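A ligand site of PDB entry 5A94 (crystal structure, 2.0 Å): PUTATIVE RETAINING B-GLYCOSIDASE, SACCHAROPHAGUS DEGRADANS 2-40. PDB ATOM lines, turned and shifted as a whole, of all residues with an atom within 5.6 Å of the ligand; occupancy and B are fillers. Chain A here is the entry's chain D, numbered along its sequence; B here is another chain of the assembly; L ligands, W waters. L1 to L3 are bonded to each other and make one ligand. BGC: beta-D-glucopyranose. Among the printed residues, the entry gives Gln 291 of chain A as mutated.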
ATOM      1  N   HIS A 107     -16.787 -34.524  -6.548  1.00  0.00           N
ATOM      2  CA  HIS A 107     -16.465 -33.155  -6.903  1.00  0.00           C
ATOM      3  C   HIS A 107     -16.651 -32.966  -8.391  1.00  0.00           C
ATOM      4  O   HIS A 107     -16.200 -33.822  -9.167  1.00  0.00           O
ATOM      5  CB  HIS A 107     -15.013 -32.828  -6.499  1.00  0.00           C
ATOM      6  CG  HIS A 107     -14.816 -32.681  -5.033  1.00  0.00           C
ATOM      7  ND1 HIS A 107     -15.216 -33.641  -4.128  1.00  0.00           N
ATOM      8  CD2 HIS A 107     -14.258 -31.693  -4.290  1.00  0.00           C
ATOM      9  CE1 HIS A 107     -14.921 -33.240  -2.908  1.00  0.00           C
ATOM     10  NE2 HIS A 107     -14.334 -32.064  -2.981  1.00  0.00           N
ATOM     11  N   HIS A 142     -20.845 -32.881  -4.832  1.00  0.00           N
ATOM     12  CA  HIS A 142     -20.119 -32.093  -3.883  1.00  0.00           C
ATOM     13  C   HIS A 142     -19.684 -30.759  -4.447  1.00  0.00           C
ATOM     14  O   HIS A 142     -18.516 -30.576  -4.776  1.00  0.00           O
ATOM     15  CB  HIS A 142     -18.928 -32.873  -3.316  1.00  0.00           C
ATOM     16  CG  HIS A 142     -18.441 -32.342  -2.003  1.00  0.00           C
ATOM     17  ND1 HIS A 142     -19.014 -32.687  -0.810  1.00  0.00           N
ATOM     18  CD2 HIS A 142     -17.422 -31.489  -1.713  1.00  0.00           C
ATOM     19  CE1 HIS A 142     -18.373 -32.073   0.173  1.00  0.00           C
ATOM     20  NE2 HIS A 142     -17.416 -31.334  -0.348  1.00  0.00           N
ATOM     21  N   ILE A 144     -20.026 -26.345  -3.686  1.00  0.00           N
ATOM     22  CA  ILE A 144     -20.236 -25.332  -2.660  1.00  0.00           C
ATOM     23  C   ILE A 144     -20.454 -23.998  -3.363  1.00  0.00           C
ATOM     24  O   ILE A 144     -19.609 -23.533  -4.125  1.00  0.00           O
ATOM     25  CB  ILE A 144     -19.018 -25.199  -1.700  1.00  0.00           C
ATOM     26  CG1 ILE A 144     -18.626 -26.559  -1.110  1.00  0.00           C
ATOM     27  CG2 ILE A 144     -19.343 -24.210  -0.597  1.00  0.00           C
ATOM     28  CD1 ILE A 144     -17.387 -26.506  -0.253  1.00  0.00           C
ATOM     29  N   MET A 156     -12.863 -26.073  -7.982  1.00  0.00           N
ATOM     30  CA  MET A 156     -13.014 -27.516  -7.855  1.00  0.00           C
ATOM     31  C   MET A 156     -14.515 -27.890  -7.721  1.00  0.00           C
ATOM     32  O   MET A 156     -14.891 -29.028  -7.981  1.00  0.00           O
ATOM     33  CB  MET A 156     -12.216 -28.061  -6.682  1.00  0.00           C
ATOM     34  CG  MET A 156     -12.729 -27.715  -5.281  1.00  0.00           C
ATOM     35  SD  MET A 156     -11.850 -28.606  -3.989  1.00  0.00           S
ATOM     36  CE  MET A 156     -10.277 -27.730  -3.905  1.00  0.00           C
ATOM     37  N   TYR A 157     -15.340 -26.914  -7.342  1.00  0.00           N
ATOM     38  CA  TYR A 157     -16.786 -27.103  -7.193  1.00  0.00           C
ATOM     39  C   TYR A 157     -17.585 -26.571  -8.372  1.00  0.00           C
ATOM     40  O   TYR A 157     -18.831 -26.674  -8.410  1.00  0.00           O
ATOM     41  CB  TYR A 157     -17.277 -26.416  -5.908  1.00  0.00           C
ATOM     42  CG  TYR A 157     -16.464 -26.773  -4.687  1.00  0.00           C
ATOM     43  CD1 TYR A 157     -16.358 -28.080  -4.236  1.00  0.00           C
ATOM     44  CD2 TYR A 157     -15.811 -25.776  -3.965  1.00  0.00           C
ATOM     45  CE1 TYR A 157     -15.613 -28.400  -3.088  1.00  0.00           C
ATOM     46  CE2 TYR A 157     -15.056 -26.075  -2.831  1.00  0.00           C
ATOM     47  CZ  TYR A 157     -14.956 -27.390  -2.411  1.00  0.00           C
ATOM     48  OH  TYR A 157     -14.181 -27.678  -1.318  1.00  0.00           O
ATOM     49  N   ASN A 188     -24.264 -30.419  -2.288  1.00  0.00           N
ATOM     50  CA  ASN A 188     -23.669 -30.475  -0.967  1.00  0.00           C
ATOM     51  C   ASN A 188     -23.907 -29.248  -0.061  1.00  0.00           C
ATOM     52  O   ASN A 188     -24.504 -29.376   1.020  1.00  0.00           O
ATOM     53  CB  ASN A 188     -22.174 -30.783  -1.148  1.00  0.00           C
ATOM     54  CG  ASN A 188     -21.326 -30.439   0.060  1.00  0.00           C
ATOM     55  OD1 ASN A 188     -21.526 -30.973   1.165  1.00  0.00           O
ATOM     56  ND2 ASN A 188     -20.305 -29.614  -0.154  1.00  0.00           N
ATOM     57  N   GLU A 189     -23.439 -28.082  -0.501  1.00  0.00           N
ATOM     58  CA  GLU A 189     -23.465 -26.889   0.346  1.00  0.00           C
ATOM     59  C   GLU A 189     -23.922 -25.605  -0.347  1.00  0.00           C
ATOM     60  O   GLU A 189     -23.100 -24.826  -0.857  1.00  0.00           O
ATOM     61  CB  GLU A 189     -22.091 -26.693   1.031  1.00  0.00           C
ATOM     62  CG  GLU A 189     -21.960 -27.581   2.262  1.00  0.00           C
ATOM     63  CD  GLU A 189     -20.673 -27.422   3.025  1.00  0.00           C
ATOM     64  OE1 GLU A 189     -19.705 -26.822   2.492  1.00  0.00           O
ATOM     65  OE2 GLU A 189     -20.622 -27.877   4.185  1.00  0.00           O
ATOM     66  N   TRP A 232     -24.114 -22.797   3.886  1.00  0.00           N
ATOM     67  CA  TRP A 232     -23.353 -24.049   3.743  1.00  0.00           C
ATOM     68  C   TRP A 232     -24.113 -25.243   4.339  1.00  0.00           C
ATOM     69  O   TRP A 232     -23.571 -26.013   5.126  1.00  0.00           O
ATOM     70  CB  TRP A 232     -21.972 -23.946   4.389  1.00  0.00           C
ATOM     71  CG  TRP A 232     -21.007 -23.070   3.684  1.00  0.00           C
ATOM     72  CD1 TRP A 232     -20.057 -23.468   2.800  1.00  0.00           C
ATOM     73  CD2 TRP A 232     -20.866 -21.642   3.812  1.00  0.00           C
ATOM     74  NE1 TRP A 232     -19.334 -22.383   2.368  1.00  0.00           N
ATOM     75  CE2 TRP A 232     -19.817 -21.252   2.965  1.00  0.00           C
ATOM     76  CE3 TRP A 232     -21.527 -20.664   4.550  1.00  0.00           C
ATOM     77  CZ2 TRP A 232     -19.405 -19.921   2.844  1.00  0.00           C
ATOM     78  CZ3 TRP A 232     -21.123 -19.327   4.419  1.00  0.00           C
ATOM     79  CH2 TRP A 232     -20.058 -18.976   3.565  1.00  0.00           C
ATOM     80  N   HIS A 254     -25.371 -29.506   8.240  1.00  0.00           N
ATOM     81  CA  HIS A 254     -23.911 -29.519   8.398  1.00  0.00           C
ATOM     82  C   HIS A 254     -23.567 -28.707   9.643  1.00  0.00           C
ATOM     83  O   HIS A 254     -23.028 -27.603   9.566  1.00  0.00           O
ATOM     84  CB  HIS A 254     -23.210 -28.943   7.161  1.00  0.00           C
ATOM     85  CG  HIS A 254     -23.233 -29.847   5.966  1.00  0.00           C
ATOM     86  ND1 HIS A 254     -22.462 -29.611   4.851  1.00  0.00           N
ATOM     87  CD2 HIS A 254     -23.929 -30.980   5.704  1.00  0.00           C
ATOM     88  CE1 HIS A 254     -22.685 -30.558   3.948  1.00  0.00           C
ATOM     89  NE2 HIS A 254     -23.559 -31.400   4.452  1.00  0.00           N
ATOM     90  N   TYR A 256     -21.311 -27.947  11.915  1.00  0.00           N
ATOM     91  CA  TYR A 256     -19.932 -27.796  12.372  1.00  0.00           C
ATOM     92  C   TYR A 256     -19.872 -26.970  13.651  1.00  0.00           C
ATOM     93  O   TYR A 256     -20.764 -26.165  13.893  1.00  0.00           O
ATOM     94  CB  TYR A 256     -19.068 -27.157  11.271  1.00  0.00           C
ATOM     95  CG  TYR A 256     -18.581 -28.140  10.232  1.00  0.00           C
ATOM     96  CD1 TYR A 256     -17.891 -29.277  10.608  1.00  0.00           C
ATOM     97  CD2 TYR A 256     -18.797 -27.925   8.873  1.00  0.00           C
ATOM     98  CE1 TYR A 256     -17.406 -30.160   9.689  1.00  0.00           C
ATOM     99  CE2 TYR A 256     -18.323 -28.820   7.916  1.00  0.00           C
ATOM    100  CZ  TYR A 256     -17.626 -29.944   8.343  1.00  0.00           C
ATOM    101  OH  TYR A 256     -17.139 -30.852   7.457  1.00  0.00           O
ATOM    102  N   GLN A 291     -22.290 -33.703   7.030  1.00  0.00           N
ATOM    103  CA  GLN A 291     -20.968 -33.235   7.450  1.00  0.00           C
ATOM    104  C   GLN A 291     -21.005 -32.735   8.882  1.00  0.00           C
ATOM    105  O   GLN A 291     -21.890 -31.955   9.254  1.00  0.00           O
ATOM    106  CB  GLN A 291     -20.435 -32.168   6.523  1.00  0.00           C
ATOM    107  CG  GLN A 291     -19.976 -32.755   5.203  1.00  0.00           C
ATOM    108  CD  GLN A 291     -19.248 -31.799   4.296  1.00  0.00           C
ATOM    109  OE1 GLN A 291     -19.443 -31.837   3.089  1.00  0.00           O
ATOM    110  NE2 GLN A 291     -18.402 -30.951   4.857  1.00  0.00           N
ATOM    111  N   TYR A 300      -3.985 -29.562  12.828  1.00  0.00           N
ATOM    112  CA  TYR A 300      -3.812 -29.671  11.378  1.00  0.00           C
ATOM    113  C   TYR A 300      -5.084 -29.292  10.631  1.00  0.00           C
ATOM    114  O   TYR A 300      -6.169 -29.787  10.930  1.00  0.00           O
ATOM    115  CB  TYR A 300      -3.438 -31.109  10.995  1.00  0.00           C
ATOM    116  CG  TYR A 300      -3.460 -31.350   9.503  1.00  0.00           C
ATOM    117  CD1 TYR A 300      -2.553 -30.727   8.666  1.00  0.00           C
ATOM    118  CD2 TYR A 300      -4.432 -32.170   8.928  1.00  0.00           C
ATOM    119  CE1 TYR A 300      -2.592 -30.929   7.290  1.00  0.00           C
ATOM    120  CE2 TYR A 300      -4.476 -32.382   7.560  1.00  0.00           C
ATOM    121  CZ  TYR A 300      -3.553 -31.771   6.743  1.00  0.00           C
ATOM    122  OH  TYR A 300      -3.607 -31.956   5.369  1.00  0.00           O
ATOM    123  N   GLY A 301      -4.928 -28.402   9.650  1.00  0.00           N
ATOM    124  CA  GLY A 301      -6.033 -27.963   8.807  1.00  0.00           C
ATOM    125  C   GLY A 301      -7.163 -27.248   9.542  1.00  0.00           C
ATOM    126  O   GLY A 301      -8.264 -27.171   9.029  1.00  0.00           O
ATOM    127  N   HIS A 303      -9.559 -24.455  10.739  1.00  0.00           N
ATOM    128  CA  HIS A 303     -10.103 -23.226  10.192  1.00  0.00           C
ATOM    129  C   HIS A 303     -11.540 -23.105  10.674  1.00  0.00           C
ATOM    130  O   HIS A 303     -12.144 -24.093  11.058  1.00  0.00           O
ATOM    131  CB  HIS A 303     -10.080 -23.244   8.656  1.00  0.00           C
ATOM    132  CG  HIS A 303     -10.815 -24.415   8.066  1.00  0.00           C
ATOM    133  ND1 HIS A 303     -10.254 -25.667   7.951  1.00  0.00           N
ATOM    134  CD2 HIS A 303     -12.081 -24.529   7.590  1.00  0.00           C
ATOM    135  CE1 HIS A 303     -11.131 -26.497   7.424  1.00  0.00           C
ATOM    136  NE2 HIS A 303     -12.252 -25.838   7.198  1.00  0.00           N
ATOM    137  N   ILE A 304     -12.086 -21.902  10.629  1.00  0.00           N
ATOM    138  CA  ILE A 304     -13.504 -21.705  10.872  1.00  0.00           C
ATOM    139  C   ILE A 304     -14.271 -22.393   9.746  1.00  0.00           C
ATOM    140  O   ILE A 304     -13.876 -22.244   8.589  1.00  0.00           O
ATOM    141  CB  ILE A 304     -13.849 -20.200  10.954  1.00  0.00           C
ATOM    142  CG1 ILE A 304     -13.129 -19.567  12.154  1.00  0.00           C
ATOM    143  CG2 ILE A 304     -15.355 -19.984  11.069  1.00  0.00           C
ATOM    144  CD1 ILE A 304     -13.223 -18.056  12.249  1.00  0.00           C
ATOM    145  N   PRO A 305     -15.356 -23.146  10.053  1.00  0.00           N
ATOM    146  CA  PRO A 305     -15.939 -23.296  11.368  1.00  0.00           C
ATOM    147  C   PRO A 305     -15.738 -24.665  12.034  1.00  0.00           C
ATOM    148  O   PRO A 305     -16.613 -25.089  12.783  1.00  0.00           O
ATOM    149  CB  PRO A 305     -17.426 -23.118  11.059  1.00  0.00           C
ATOM    150  CG  PRO A 305     -17.578 -23.882   9.771  1.00  0.00           C
ATOM    151  CD  PRO A 305     -16.239 -23.755   9.036  1.00  0.00           C
ATOM    152  N   VAL A 306     -14.592 -25.300  11.808  1.00  0.00           N
ATOM    153  CA  VAL A 306     -14.337 -26.637  12.381  1.00  0.00           C
ATOM    154  C   VAL A 306     -13.439 -26.642  13.642  1.00  0.00           C
ATOM    155  O   VAL A 306     -13.075 -27.699  14.123  1.00  0.00           O
ATOM    156  CB  VAL A 306     -13.754 -27.592  11.312  1.00  0.00           C
ATOM    157  CG1 VAL A 306     -14.662 -27.617  10.081  1.00  0.00           C
ATOM    158  CG2 VAL A 306     -12.334 -27.205  10.914  1.00  0.00           C
ATOM    159  N   TRP A 330     -17.134 -35.906   8.719  1.00  0.00           N
ATOM    160  CA  TRP A 330     -16.161 -35.412   7.774  1.00  0.00           C
ATOM    161  C   TRP A 330     -14.789 -35.249   8.462  1.00  0.00           C
ATOM    162  O   TRP A 330     -14.719 -34.561   9.474  1.00  0.00           O
ATOM    163  CB  TRP A 330     -16.632 -34.063   7.210  1.00  0.00           C
ATOM    164  CG  TRP A 330     -15.674 -33.515   6.240  1.00  0.00           C
ATOM    165  CD1 TRP A 330     -14.542 -32.807   6.524  1.00  0.00           C
ATOM    166  CD2 TRP A 330     -15.716 -33.642   4.811  1.00  0.00           C
ATOM    167  NE1 TRP A 330     -13.882 -32.501   5.358  1.00  0.00           N
ATOM    168  CE2 TRP A 330     -14.575 -32.999   4.296  1.00  0.00           C
ATOM    169  CE3 TRP A 330     -16.605 -34.262   3.911  1.00  0.00           C
ATOM    170  CZ2 TRP A 330     -14.290 -32.945   2.923  1.00  0.00           C
ATOM    171  CZ3 TRP A 330     -16.333 -34.178   2.546  1.00  0.00           C
ATOM    172  CH2 TRP A 330     -15.187 -33.534   2.077  1.00  0.00           C
ATOM    173  N   ASP A 335      -5.448 -36.378   4.641  1.00  0.00           N
ATOM    174  CA  ASP A 335      -5.036 -35.130   4.015  1.00  0.00           C
ATOM    175  C   ASP A 335      -6.100 -34.050   4.159  1.00  0.00           C
ATOM    176  O   ASP A 335      -5.828 -32.943   4.601  1.00  0.00           O
ATOM    177  CB  ASP A 335      -4.746 -35.336   2.526  1.00  0.00           C
ATOM    178  CG  ASP A 335      -3.709 -36.405   2.271  1.00  0.00           C
ATOM    179  OD1 ASP A 335      -2.609 -36.297   2.844  1.00  0.00           O
ATOM    180  OD2 ASP A 335      -3.980 -37.349   1.517  1.00  0.00           O
ATOM    181  N   TRP A 336      -7.335 -34.392   3.784  1.00  0.00           N
ATOM    182  CA  TRP A 336      -8.450 -33.470   3.875  1.00  0.00           C
ATOM    183  C   TRP A 336      -8.903 -33.333   5.314  1.00  0.00           C
ATOM    184  O   TRP A 336      -8.930 -34.316   6.038  1.00  0.00           O
ATOM    185  CB  TRP A 336      -9.610 -33.973   3.009  1.00  0.00           C
ATOM    186  CG  TRP A 336      -9.386 -33.836   1.515  1.00  0.00           C
ATOM    187  CD1 TRP A 336      -8.234 -33.464   0.873  1.00  0.00           C
ATOM    188  CD2 TRP A 336     -10.352 -34.098   0.487  1.00  0.00           C
ATOM    189  NE1 TRP A 336      -8.442 -33.456  -0.505  1.00  0.00           N
ATOM    190  CE2 TRP A 336      -9.728 -33.854  -0.754  1.00  0.00           C
ATOM    191  CE3 TRP A 336     -11.701 -34.484   0.514  1.00  0.00           C
ATOM    192  CZ2 TRP A 336     -10.408 -33.998  -1.957  1.00  0.00           C
ATOM    193  CZ3 TRP A 336     -12.361 -34.628  -0.675  1.00  0.00           C
ATOM    194  CH2 TRP A 336     -11.724 -34.386  -1.899  1.00  0.00           C
ATOM    195  N   SER A 337      -9.261 -32.106   5.690  1.00  0.00           N
ATOM    196  CA  SER A 337      -9.521 -31.776   7.098  1.00  0.00           C
ATOM    197  C   SER A 337     -10.940 -31.300   7.338  1.00  0.00           C
ATOM    198  O   SER A 337     -11.594 -30.864   6.384  1.00  0.00           O
ATOM    199  CB  SER A 337      -8.510 -30.727   7.569  1.00  0.00           C
ATOM    200  OG  SER A 337      -8.654 -29.519   6.863  1.00  0.00           O
ATOM    201  N   PRO A 338     -11.427 -31.407   8.592  1.00  0.00           N
ATOM    202  CA  PRO A 338     -10.704 -32.097   9.659  1.00  0.00           C
ATOM    203  C   PRO A 338     -10.627 -33.612   9.465  1.00  0.00           C
ATOM    204  O   PRO A 338     -11.621 -34.268   9.093  1.00  0.00           O
ATOM    205  CB  PRO A 338     -11.512 -31.746  10.909  1.00  0.00           C
ATOM    206  CG  PRO A 338     -12.886 -31.562  10.386  1.00  0.00           C
ATOM    207  CD  PRO A 338     -12.691 -30.846   9.075  1.00  0.00           C
ATOM    208  N   TRP B  31      -6.121 -30.890  -8.470  1.00  0.00           N
ATOM    209  CA  TRP B  31      -7.172 -29.874  -8.344  1.00  0.00           C
ATOM    210  C   TRP B  31      -7.494 -29.491  -6.884  1.00  0.00           C
ATOM    211  O   TRP B  31      -7.780 -28.335  -6.607  1.00  0.00           O
ATOM    212  CB  TRP B  31      -8.455 -30.295  -9.075  1.00  0.00           C
ATOM    213  CG  TRP B  31      -8.977 -31.654  -8.744  1.00  0.00           C
ATOM    214  CD1 TRP B  31      -8.790 -32.796  -9.460  1.00  0.00           C
ATOM    215  CD2 TRP B  31      -9.783 -32.007  -7.610  1.00  0.00           C
ATOM    216  NE1 TRP B  31      -9.439 -33.858  -8.836  1.00  0.00           N
ATOM    217  CE2 TRP B  31     -10.063 -33.392  -7.714  1.00  0.00           C
ATOM    218  CE3 TRP B  31     -10.311 -31.291  -6.536  1.00  0.00           C
ATOM    219  CZ2 TRP B  31     -10.838 -34.076  -6.769  1.00  0.00           C
ATOM    220  CZ3 TRP B  31     -11.093 -31.969  -5.602  1.00  0.00           C
ATOM    221  CH2 TRP B  31     -11.333 -33.352  -5.716  1.00  0.00           C
ATOM    222  N   TRP B  32      -7.372 -30.446  -5.963  1.00  0.00           N
ATOM    223  CA  TRP B  32      -7.640 -30.173  -4.550  1.00  0.00           C
ATOM    224  C   TRP B  32      -6.567 -29.309  -3.881  1.00  0.00           C
ATOM    225  O   TRP B  32      -6.797 -28.786  -2.788  1.00  0.00           O
ATOM    226  CB  TRP B  32      -7.859 -31.470  -3.759  1.00  0.00           C
ATOM    227  CG  TRP B  32      -6.698 -32.447  -3.780  1.00  0.00           C
ATOM    228  CD1 TRP B  32      -5.650 -32.510  -2.899  1.00  0.00           C
ATOM    229  CD2 TRP B  32      -6.496 -33.488  -4.717  1.00  0.00           C
ATOM    230  NE1 TRP B  32      -4.799 -33.532  -3.237  1.00  0.00           N
ATOM    231  CE2 TRP B  32      -5.298 -34.157  -4.359  1.00  0.00           C
ATOM    232  CE3 TRP B  32      -7.204 -33.938  -5.839  1.00  0.00           C
ATOM    233  CZ2 TRP B  32      -4.798 -35.243  -5.082  1.00  0.00           C
ATOM    234  CZ3 TRP B  32      -6.703 -35.012  -6.556  1.00  0.00           C
ATOM    235  CH2 TRP B  32      -5.505 -35.654  -6.172  1.00  0.00           C
ATOM    236  N   ASP B  33      -5.419 -29.143  -4.522  1.00  0.00           N
ATOM    237  CA  ASP B  33      -4.360 -28.238  -4.045  1.00  0.00           C
ATOM    238  C   ASP B  33      -4.423 -26.826  -4.636  1.00  0.00           C
ATOM    239  O   ASP B  33      -3.595 -25.975  -4.286  1.00  0.00           O
ATOM    240  CB  ASP B  33      -2.986 -28.828  -4.335  1.00  0.00           C
ATOM    241  CG  ASP B  33      -2.675 -30.049  -3.511  1.00  0.00           C
ATOM    242  OD1 ASP B  33      -3.014 -30.058  -2.296  1.00  0.00           O
ATOM    243  OD2 ASP B  33      -2.064 -30.975  -4.069  1.00  0.00           O
HETATM  244  C2  BGC L   1     -16.844 -28.546   2.695  1.00  0.00           C
HETATM  245  C3  BGC L   1     -15.696 -29.562   2.661  1.00  0.00           C
HETATM  246  C4  BGC L   1     -14.510 -28.973   3.428  1.00  0.00           C
HETATM  247  C5  BGC L   1     -14.984 -28.504   4.780  1.00  0.00           C
HETATM  248  C6  BGC L   1     -13.872 -27.999   5.685  1.00  0.00           C
HETATM  249  C1  BGC L   1     -17.104 -27.866   4.071  1.00  0.00           C
HETATM  250  O1  BGC L   1     -17.863 -26.661   4.037  1.00  0.00           O
HETATM  251  O2  BGC L   1     -17.984 -29.265   2.213  1.00  0.00           O
HETATM  252  O3  BGC L   1     -15.382 -29.930   1.286  1.00  0.00           O
HETATM  253  O4  BGC L   1     -13.431 -29.912   3.573  1.00  0.00           O
HETATM  254  O5  BGC L   1     -15.857 -27.400   4.559  1.00  0.00           O
HETATM  255  O6  BGC L   1     -14.517 -27.302   6.761  1.00  0.00           O
HETATM  256  C2  BGC L   2     -11.047 -30.006   3.222  1.00  0.00           C
HETATM  257  C3  BGC L   2      -9.948 -29.649   2.237  1.00  0.00           C
HETATM  258  C4  BGC L   2     -10.240 -30.260   0.881  1.00  0.00           C
HETATM  259  C5  BGC L   2     -11.665 -29.956   0.448  1.00  0.00           C
HETATM  260  C6  BGC L   2     -12.056 -30.701  -0.809  1.00  0.00           C
HETATM  261  C1  BGC L   2     -12.400 -29.597   2.656  1.00  0.00           C
HETATM  262  O2  BGC L   2     -10.796 -29.295   4.402  1.00  0.00           O
HETATM  263  O3  BGC L   2      -8.747 -30.144   2.803  1.00  0.00           O
HETATM  264  O4  BGC L   2      -9.362 -29.720  -0.102  1.00  0.00           O
HETATM  265  O5  BGC L   2     -12.597 -30.302   1.467  1.00  0.00           O
HETATM  266  O6  BGC L   2     -13.412 -30.360  -1.125  1.00  0.00           O
HETATM  267  C2  BGC L   3      -6.593 -29.498   3.652  1.00  0.00           C
HETATM  268  C3  BGC L   3      -5.220 -28.955   3.253  1.00  0.00           C
HETATM  269  C4  BGC L   3      -4.674 -29.703   2.047  1.00  0.00           C
HETATM  270  C5  BGC L   3      -5.727 -29.792   0.963  1.00  0.00           C
HETATM  271  C6  BGC L   3      -5.480 -30.903  -0.021  1.00  0.00           C
HETATM  272  C1  BGC L   3      -7.551 -29.430   2.485  1.00  0.00           C
HETATM  273  O2  BGC L   3      -7.144 -28.717   4.713  1.00  0.00           O
HETATM  274  O3  BGC L   3      -4.262 -29.194   4.270  1.00  0.00           O
HETATM  275  O4  BGC L   3      -3.489 -29.036   1.571  1.00  0.00           O
HETATM  276  O5  BGC L   3      -7.013 -30.175   1.417  1.00  0.00           O
HETATM  277  O6  BGC L   3      -6.716 -30.918  -0.750  1.00  0.00           O
HETATM  278  O   HOH W   1     -19.778 -25.769   6.606  1.00  0.00           O
HETATM  279  O   HOH W   2      -9.293 -26.871  -0.502  1.00  0.00           O
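The side-chain carboxylate (OE1) of Glu 189 lies within hydrogen-bond range of an oxygen (O1) of BGC L1 (2.4 Å).
N of Ser 337 lies within hydrogen-bond range of O2 of BGC L2, 3.5 Å away.
The backbone carbonyl oxygen (O) of Ser 337 is in hydrogen-bond range of an oxygen (O2) of BGC L2, at 2.7 Å.
The side-chain hydroxyl (OG) of Ser 337 lies within hydrogen-bond range of an oxygen (O2) of BGC L3.
A ring nitrogen (NE2) of His 107 lies within hydrogen-bond range of an oxygen (O6) of BGC L2 (2.7 Å).
NE2 of His 303 is in hydrogen-bond range of O6 of BGC L1, at 2.7 Å.
The side-chain hydroxyl of Tyr 157 lies within hydrogen-bond range of an oxygen (O6) of BGC L2, at 2.8 Å.
O6 of BGC L3 sits close to O of Trp 32 of chain B (3.0 Å).
An oxygen (O3) of BGC L1 sits at hydrogen-bond distance from a ring nitrogen (NE2) of His 142.
OH of Tyr 300 sits at hydrogen-bond distance from O3 of BGC L3 (3.0 Å).
NE1 of Trp 336 is in hydrogen-bond range of O6 of BGC L3 (3.1 Å).
An oxygen (O2) of BGC L1 lies within hydrogen-bond range of the side-chain amide oxygen (OE1) of Gln 291.
The indole nitrogen of Trp 330 sits at hydrogen-bond distance from an oxygen (O4) of BGC L1, 3.2 Å away.
O2 of BGC L1 sits at hydrogen-bond distance from ND2 of Asn 188 (3.3 Å).
SD of Met 156 is in hydrogen-bond range of O6 of BGC L2 (3.7 Å).
OE2 of Glu 189 sits at hydrogen-bond distance from ND1 of His 254, 2.6 Å away.
The side-chain hydroxyl (OG) of Ser 337 lies within hydrogen-bond range of the backbone carbonyl oxygen (O) of Gly 301 (3.2 Å).
A ring nitrogen (ND1) of His 303 lies within hydrogen-bond range of the backbone carbonyl oxygen of Gly 301 (2.7 Å).
The side-chain sulfur of Met 156 lies within hydrogen-bond range of the side-chain hydroxyl of Tyr 157, at 3.7 Å.
NE2 of His 142 lies close to ND2 of Asn 188, 3.4 Å away.
The side-chain hydroxyl (OH) of Tyr 300 lies within hydrogen-bond range of the backbone carbonyl oxygen (O) of Asp 335 (2.5 Å).
The side-chain amide oxygen of Asn 188 lies close to the side-chain amide oxygen of Gln 291, 3.0 Å away.
The side-chain amide nitrogen (NE2) of Gln 291 sits at hydrogen-bond distance from the side-chain hydroxyl (OH) of Tyr 256, 2.9 Å away.
Residues that only touch the ligand: Val 306, Asp 33 of chain B, Ile 144 and Asp 335.
Of the 25 residues printed, 17 come within 4 Å of the ligand.
Water W1 lies within hydrogen-bond range of OE2 of Glu 189 (3.3 Å) and O1 of BGC L1 (3.3 Å).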
